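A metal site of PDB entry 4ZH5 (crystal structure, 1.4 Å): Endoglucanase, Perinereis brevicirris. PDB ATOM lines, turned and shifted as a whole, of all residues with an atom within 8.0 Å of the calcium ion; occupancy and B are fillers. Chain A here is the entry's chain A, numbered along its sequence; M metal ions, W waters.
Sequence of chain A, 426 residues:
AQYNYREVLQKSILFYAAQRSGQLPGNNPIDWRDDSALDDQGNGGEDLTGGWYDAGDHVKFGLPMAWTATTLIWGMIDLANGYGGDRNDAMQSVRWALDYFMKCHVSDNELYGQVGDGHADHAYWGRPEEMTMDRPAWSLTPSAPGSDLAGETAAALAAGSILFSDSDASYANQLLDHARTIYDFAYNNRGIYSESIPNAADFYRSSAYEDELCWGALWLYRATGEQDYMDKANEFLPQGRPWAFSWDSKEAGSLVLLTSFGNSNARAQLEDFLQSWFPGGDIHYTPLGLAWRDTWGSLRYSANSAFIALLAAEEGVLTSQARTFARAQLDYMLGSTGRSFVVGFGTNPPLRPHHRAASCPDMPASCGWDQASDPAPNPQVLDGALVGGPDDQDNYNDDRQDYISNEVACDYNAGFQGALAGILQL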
ATOM      1  N   LEU A  63      -3.583 -28.350 -12.543  1.00  0.00           N
ATOM      2  CA  LEU A  63      -3.507 -28.025 -13.973  1.00  0.00           C
ATOM      3  C   LEU A  63      -4.457 -28.867 -14.824  1.00  0.00           C
ATOM      4  O   LEU A  63      -5.298 -28.314 -15.513  1.00  0.00           O
ATOM      5  CB  LEU A  63      -2.083 -28.072 -14.459  1.00  0.00           C
ATOM      6  CG  LEU A  63      -1.882 -27.786 -15.964  1.00  0.00           C
ATOM      7  CD1 LEU A  63      -2.436 -26.420 -16.383  1.00  0.00           C
ATOM      8  CD2 LEU A  63      -0.425 -27.862 -16.376  1.00  0.00           C
ATOM      9  N   SER A 147       2.233 -19.516 -13.917  1.00  0.00           N
ATOM     10  CA  SER A 147       1.372 -18.851 -14.880  1.00  0.00           C
ATOM     11  C   SER A 147       0.523 -19.795 -15.676  1.00  0.00           C
ATOM     12  O   SER A 147      -0.557 -19.436 -16.176  1.00  0.00           O
ATOM     13  CB  SER A 147       2.225 -18.043 -15.837  1.00  0.00           C
ATOM     14  OG  SER A 147       3.073 -17.131 -15.139  1.00  0.00           O
ATOM     15  N   ASP A 148       1.028 -21.031 -15.808  1.00  0.00           N
ATOM     16  CA  ASP A 148       0.335 -22.107 -16.477  1.00  0.00           C
ATOM     17  C   ASP A 148      -0.912 -22.584 -15.673  1.00  0.00           C
ATOM     18  O   ASP A 148      -2.047 -22.465 -16.140  1.00  0.00           O
ATOM     19  CB  ASP A 148       1.297 -23.290 -16.788  1.00  0.00           C
ATOM     20  CG  ASP A 148       2.388 -23.510 -15.760  1.00  0.00           C
ATOM     21  OD1 ASP A 148       2.184 -23.119 -14.566  1.00  0.00           O
ATOM     22  OD2 ASP A 148       3.472 -24.027 -16.141  1.00  0.00           O
ATOM     23  N   LEU A 149      -0.690 -23.058 -14.448  1.00  0.00           N
ATOM     24  CA  LEU A 149      -1.805 -23.512 -13.622  1.00  0.00           C
ATOM     25  C   LEU A 149      -2.771 -22.370 -13.344  1.00  0.00           C
ATOM     26  O   LEU A 149      -3.983 -22.519 -13.443  1.00  0.00           O
ATOM     27  CB  LEU A 149      -1.285 -24.180 -12.347  1.00  0.00           C
ATOM     28  CG  LEU A 149      -2.329 -24.861 -11.471  1.00  0.00           C
ATOM     29  CD1 LEU A 149      -1.678 -26.019 -10.691  1.00  0.00           C
ATOM     30  CD2 LEU A 149      -3.064 -23.937 -10.507  1.00  0.00           C
ATOM     31  N   GLU A 152      -4.695 -21.332 -16.553  1.00  0.00           N
ATOM     32  CA  GLU A 152      -5.744 -22.307 -16.848  1.00  0.00           C
ATOM     33  C   GLU A 152      -6.927 -22.228 -15.878  1.00  0.00           C
ATOM     34  O   GLU A 152      -8.072 -22.370 -16.307  1.00  0.00           O
ATOM     35  CB  GLU A 152      -5.173 -23.731 -16.805  1.00  0.00           C
ATOM     36  CG  GLU A 152      -6.193 -24.772 -17.302  1.00  0.00           C
ATOM     37  CD  GLU A 152      -6.487 -24.636 -18.768  1.00  0.00           C
ATOM     38  OE1 GLU A 152      -5.519 -24.619 -19.529  1.00  0.00           O
ATOM     39  OE2 GLU A 152      -7.684 -24.505 -19.140  1.00  0.00           O
ATOM     40  N   ILE A 192       6.821 -21.462 -14.198  1.00  0.00           N
ATOM     41  CA  ILE A 192       6.277 -22.815 -14.438  1.00  0.00           C
ATOM     42  C   ILE A 192       5.833 -23.375 -13.090  1.00  0.00           C
ATOM     43  O   ILE A 192       6.645 -23.522 -12.159  1.00  0.00           O
ATOM     44  CB  ILE A 192       7.392 -23.682 -15.057  1.00  0.00           C
ATOM     45  CG1 ILE A 192       7.756 -23.176 -16.449  1.00  0.00           C
ATOM     46  CG2 ILE A 192       7.004 -25.133 -15.097  1.00  0.00           C
ATOM     47  CD1 ILE A 192       6.752 -23.550 -17.518  1.00  0.00           C
ATOM     48  N   ARG A 205       4.163 -32.393 -15.381  1.00  0.00           N
ATOM     49  CA  ARG A 205       5.219 -31.460 -15.703  1.00  0.00           C
ATOM     50  C   ARG A 205       4.730 -30.503 -16.796  1.00  0.00           C
ATOM     51  O   ARG A 205       4.363 -30.925 -17.881  1.00  0.00           O
ATOM     52  CB  ARG A 205       6.440 -32.203 -16.218  1.00  0.00           C
ATOM     53  CG  ARG A 205       7.613 -31.319 -16.583  1.00  0.00           C
ATOM     54  CD  ARG A 205       8.576 -32.227 -17.278  1.00  0.00           C
ATOM     55  NE  ARG A 205       9.763 -31.532 -17.739  1.00  0.00           N
ATOM     56  CZ  ARG A 205      10.620 -32.042 -18.613  1.00  0.00           C
ATOM     57  NH1 ARG A 205      10.479 -33.297 -19.063  1.00  0.00           N
ATOM     58  NH2 ARG A 205      11.659 -31.368 -18.955  1.00  0.00           N
ATOM     59  N   SER A 206       4.797 -29.205 -16.543  1.00  0.00           N
ATOM     60  CA  SER A 206       4.401 -28.224 -17.554  1.00  0.00           C
ATOM     61  C   SER A 206       5.541 -27.923 -18.492  1.00  0.00           C
ATOM     62  O   SER A 206       6.636 -27.617 -18.047  1.00  0.00           O
ATOM     63  CB  SER A 206       3.929 -26.978 -16.868  1.00  0.00           C
ATOM     64  OG  SER A 206       3.767 -25.947 -17.828  1.00  0.00           O
ATOM     65  N   SER A 207       5.267 -27.989 -19.800  1.00  0.00           N
ATOM     66  CA  SER A 207       6.296 -27.701 -20.789  1.00  0.00           C
ATOM     67  C   SER A 207       6.476 -26.201 -21.073  1.00  0.00           C
ATOM     68  O   SER A 207       7.531 -25.794 -21.561  1.00  0.00           O
ATOM     69  CB  SER A 207       6.053 -28.464 -22.073  1.00  0.00           C
ATOM     70  OG  SER A 207       4.801 -28.169 -22.655  1.00  0.00           O
ATOM     71  N   ALA A 208       5.473 -25.400 -20.778  1.00  0.00           N
ATOM     72  CA  ALA A 208       5.509 -23.957 -21.092  1.00  0.00           C
ATOM     73  C   ALA A 208       4.256 -23.340 -20.484  1.00  0.00           C
ATOM     74  O   ALA A 208       3.239 -24.013 -20.360  1.00  0.00           O
ATOM     75  CB  ALA A 208       5.516 -23.720 -22.575  1.00  0.00           C
ATOM     76  N   TYR A 209       4.335 -22.042 -20.166  1.00  0.00           N
ATOM     77  CA  TYR A 209       3.198 -21.313 -19.685  1.00  0.00           C
ATOM     78  C   TYR A 209       2.604 -20.263 -20.599  1.00  0.00           C
ATOM     79  O   TYR A 209       1.497 -19.814 -20.364  1.00  0.00           O
ATOM     80  CB  TYR A 209       3.483 -20.690 -18.311  1.00  0.00           C
ATOM     81  CG  TYR A 209       4.557 -19.643 -18.342  1.00  0.00           C
ATOM     82  CD1 TYR A 209       4.341 -18.397 -18.903  1.00  0.00           C
ATOM     83  CD2 TYR A 209       5.807 -19.933 -17.809  1.00  0.00           C
ATOM     84  CE1 TYR A 209       5.356 -17.464 -18.936  1.00  0.00           C
ATOM     85  CE2 TYR A 209       6.824 -18.984 -17.823  1.00  0.00           C
ATOM     86  CZ  TYR A 209       6.593 -17.755 -18.406  1.00  0.00           C
ATOM     87  OH  TYR A 209       7.600 -16.801 -18.441  1.00  0.00           O
ATOM     88  N   GLU A 210       3.313 -19.867 -21.646  1.00  0.00           N
ATOM     89  CA  GLU A 210       2.775 -18.755 -22.456  1.00  0.00           C
ATOM     90  C   GLU A 210       1.500 -19.171 -23.194  1.00  0.00           C
ATOM     91  O   GLU A 210       0.624 -18.322 -23.458  1.00  0.00           O
ATOM     92  CB  GLU A 210       3.824 -18.176 -23.389  1.00  0.00           C
ATOM     93  CG  GLU A 210       4.842 -17.321 -22.654  1.00  0.00           C
ATOM     94  CD  GLU A 210       5.610 -16.391 -23.537  1.00  0.00           C
ATOM     95  OE1 GLU A 210       6.102 -15.355 -23.013  1.00  0.00           O
ATOM     96  OE2 GLU A 210       5.769 -16.684 -24.722  1.00  0.00           O
ATOM     97  N   ASP A 211       1.356 -20.459 -23.488  1.00  0.00           N
ATOM     98  CA  ASP A 211       0.107 -20.909 -24.100  1.00  0.00           C
ATOM     99  C   ASP A 211      -1.079 -20.773 -23.181  1.00  0.00           C
ATOM    100  O   ASP A 211      -2.173 -20.437 -23.654  1.00  0.00           O
ATOM    101  CB  ASP A 211       0.182 -22.324 -24.667  1.00  0.00           C
ATOM    102  CG  ASP A 211       0.684 -23.353 -23.632  1.00  0.00           C
ATOM    103  OD1 ASP A 211       1.778 -23.187 -23.071  1.00  0.00           O
ATOM    104  OD2 ASP A 211      -0.075 -24.352 -23.419  1.00  0.00           O
ATOM    105  N   GLU A 212      -0.880 -20.967 -21.870  1.00  0.00           N
ATOM    106  CA  GLU A 212      -1.969 -20.693 -20.907  1.00  0.00           C
ATOM    107  C   GLU A 212      -2.242 -19.188 -20.767  1.00  0.00           C
ATOM    108  O   GLU A 212      -3.361 -18.811 -20.527  1.00  0.00           O
ATOM    109  CB  GLU A 212      -1.692 -21.280 -19.536  1.00  0.00           C
ATOM    110  CG  GLU A 212      -1.852 -22.823 -19.479  1.00  0.00           C
ATOM    111  CD  GLU A 212      -0.704 -23.587 -20.100  1.00  0.00           C
ATOM    112  OE1 GLU A 212       0.393 -23.041 -20.282  1.00  0.00           O
ATOM    113  OE2 GLU A 212      -0.908 -24.806 -20.380  1.00  0.00           O
ATOM    114  N   LEU A 213      -1.190 -18.370 -20.860  1.00  0.00           N
ATOM    115  CA  LEU A 213      -1.416 -16.913 -20.829  1.00  0.00           C
ATOM    116  C   LEU A 213      -2.272 -16.485 -22.036  1.00  0.00           C
ATOM    117  O   LEU A 213      -3.135 -15.609 -21.919  1.00  0.00           O
ATOM    118  CB  LEU A 213      -0.119 -16.138 -20.705  1.00  0.00           C
ATOM    119  CG  LEU A 213       0.572 -16.292 -19.351  1.00  0.00           C
ATOM    120  CD1 LEU A 213       1.877 -15.501 -19.369  1.00  0.00           C
ATOM    121  CD2 LEU A 213      -0.299 -15.849 -18.196  1.00  0.00           C
ATOM    122  N   SER A 246      -4.125 -30.726 -25.187  1.00  0.00           N
ATOM    123  CA  SER A 246      -4.104 -31.503 -23.943  1.00  0.00           C
ATOM    124  C   SER A 246      -4.078 -30.576 -22.760  1.00  0.00           C
ATOM    125  O   SER A 246      -4.013 -29.337 -22.921  1.00  0.00           O
ATOM    126  CB  SER A 246      -2.826 -32.379 -23.886  1.00  0.00           C
ATOM    127  OG  SER A 246      -1.677 -31.596 -23.653  1.00  0.00           O
ATOM    128  N   TRP A 247      -4.022 -31.145 -21.551  1.00  0.00           N
ATOM    129  CA  TRP A 247      -3.823 -30.404 -20.341  1.00  0.00           C
ATOM    130  C   TRP A 247      -2.537 -29.569 -20.326  1.00  0.00           C
ATOM    131  O   TRP A 247      -2.448 -28.665 -19.534  1.00  0.00           O
ATOM    132  CB  TRP A 247      -3.854 -31.372 -19.141  1.00  0.00           C
ATOM    133  CG  TRP A 247      -2.717 -32.342 -19.163  1.00  0.00           C
ATOM    134  CD1 TRP A 247      -2.746 -33.608 -19.701  1.00  0.00           C
ATOM    135  CD2 TRP A 247      -1.359 -32.128 -18.750  1.00  0.00           C
ATOM    136  NE1 TRP A 247      -1.515 -34.166 -19.641  1.00  0.00           N
ATOM    137  CE2 TRP A 247      -0.639 -33.305 -19.064  1.00  0.00           C
ATOM    138  CE3 TRP A 247      -0.682 -31.086 -18.122  1.00  0.00           C
ATOM    139  CZ2 TRP A 247       0.719 -33.452 -18.794  1.00  0.00           C
ATOM    140  CZ3 TRP A 247       0.653 -31.233 -17.851  1.00  0.00           C
ATOM    141  CH2 TRP A 247       1.341 -32.382 -18.213  1.00  0.00           C
ATOM    142  N   ASP A 248      -1.563 -29.942 -21.119  1.00  0.00           N
ATOM    143  CA  ASP A 248      -0.264 -29.268 -21.146  1.00  0.00           C
ATOM    144  C   ASP A 248      -0.225 -28.153 -22.215  1.00  0.00           C
ATOM    145  O   ASP A 248       0.373 -27.156 -21.996  1.00  0.00           O
ATOM    146  CB  ASP A 248       0.868 -30.296 -21.413  1.00  0.00           C
ATOM    147  CG  ASP A 248       2.234 -29.698 -21.373  1.00  0.00           C
ATOM    148  OD1 ASP A 248       2.547 -28.942 -20.429  1.00  0.00           O
ATOM    149  OD2 ASP A 248       3.017 -30.028 -22.281  1.00  0.00           O
ATOM    150  N   SER A 249      -0.747 -28.445 -23.404  1.00  0.00           N
ATOM    151  CA  SER A 249      -0.674 -27.556 -24.582  1.00  0.00           C
ATOM    152  C   SER A 249      -2.017 -26.992 -24.963  1.00  0.00           C
ATOM    153  O   SER A 249      -2.904 -27.722 -25.393  1.00  0.00           O
ATOM    154  CB  SER A 249      -0.162 -28.326 -25.809  1.00  0.00           C
ATOM    155  OG  SER A 249       1.195 -28.697 -25.712  1.00  0.00           O
ATOM    156  N   LYS A 250      -2.161 -25.661 -24.859  1.00  0.00           N
ATOM    157  CA  LYS A 250      -3.416 -25.006 -25.175  1.00  0.00           C
ATOM    158  C   LYS A 250      -3.507 -24.436 -26.580  1.00  0.00           C
ATOM    159  O   LYS A 250      -4.587 -23.978 -26.966  1.00  0.00           O
ATOM    160  CB  LYS A 250      -3.714 -23.890 -24.156  1.00  0.00           C
ATOM    161  CG  LYS A 250      -3.554 -24.265 -22.696  1.00  0.00           C
ATOM    162  CD  LYS A 250      -4.418 -25.490 -22.376  1.00  0.00           C
ATOM    163  CE  LYS A 250      -3.678 -26.537 -21.537  1.00  0.00           C
ATOM    164  NZ  LYS A 250      -3.337 -26.010 -20.193  1.00  0.00           N
ATOM    165  N   GLU A 251      -2.404 -24.441 -27.296  1.00  0.00           N
ATOM    166  CA  GLU A 251      -2.352 -23.705 -28.560  1.00  0.00           C
ATOM    167  C   GLU A 251      -3.484 -24.057 -29.511  1.00  0.00           C
ATOM    168  O   GLU A 251      -4.029 -23.151 -30.146  1.00  0.00           O
ATOM    169  CB  GLU A 251      -1.017 -23.949 -29.246  1.00  0.00           C
ATOM    170  CG  GLU A 251       0.194 -23.307 -28.562  1.00  0.00           C
ATOM    171  CD  GLU A 251       0.955 -24.138 -27.573  1.00  0.00           C
ATOM    172  OE1 GLU A 251       0.355 -24.957 -26.848  1.00  0.00           O
ATOM    173  OE2 GLU A 251       2.188 -23.910 -27.486  1.00  0.00           O
HETATM  174 CA    CA M   1       1.300 -25.027 -21.424  1.00  0.00          CA
HETATM  175  O   HOH W   1       1.783 -26.450 -19.561  1.00  0.00           O
HETATM  176  O   HOH W   2       2.970 -26.033 -22.872  1.00  0.00           O
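OD2 of Asp 248 sits at hydrogen-bond distance from OG of Ser 207 (2.6 Å). The backbone NH (N) of Asp 248 lies within hydrogen-bond range of the side-chain hydroxyl (OG) of Ser 246 (3.0 Å). The backbone NH of Ala 208 lies close to the side-chain hydroxyl of Ser 206. NZ of Lys 250 lies close to OE2 of Glu 212. The backbone NH of Lys 250 sits close to the side-chain carboxylate of Asp 211.
Within 4 Å of the calcium ion: Ala 208, Asp 211, Glu 212 and Asp 248. Along chain A the residues within 4 Å of the calcium ion span positions 208 to 248. The nearest printed residue that does not touch the calcium ion is Tyr 209 (4.4 Å).
The calcium ion is bound by the backbone carbonyl oxygen (O) of Asp 248 (2.4 Å), water W1 (2.4 Å), water W2 (2.4 Å), the backbone carbonyl oxygen (O) of Ala 208 (2.4 Å), the side-chain carboxylate (OE2) of Glu 212 (2.5 Å), the side-chain carboxylate (OE1) of Glu 212 (2.5 Å), the side-chain carboxylate (OD1) of Asp 211 (2.5 Å) and the side-chain carboxylate (OD2) of Asp 211 (2.5 Å).
Water W2 lies within hydrogen-bond range of the side-chain hydroxyl of Ser 207 and the backbone NH of Ala 208. Water W1 bridges the side-chain hydroxyl (OG) of Ser 206 and the side-chain carboxylate (OD1) of Asp 248.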
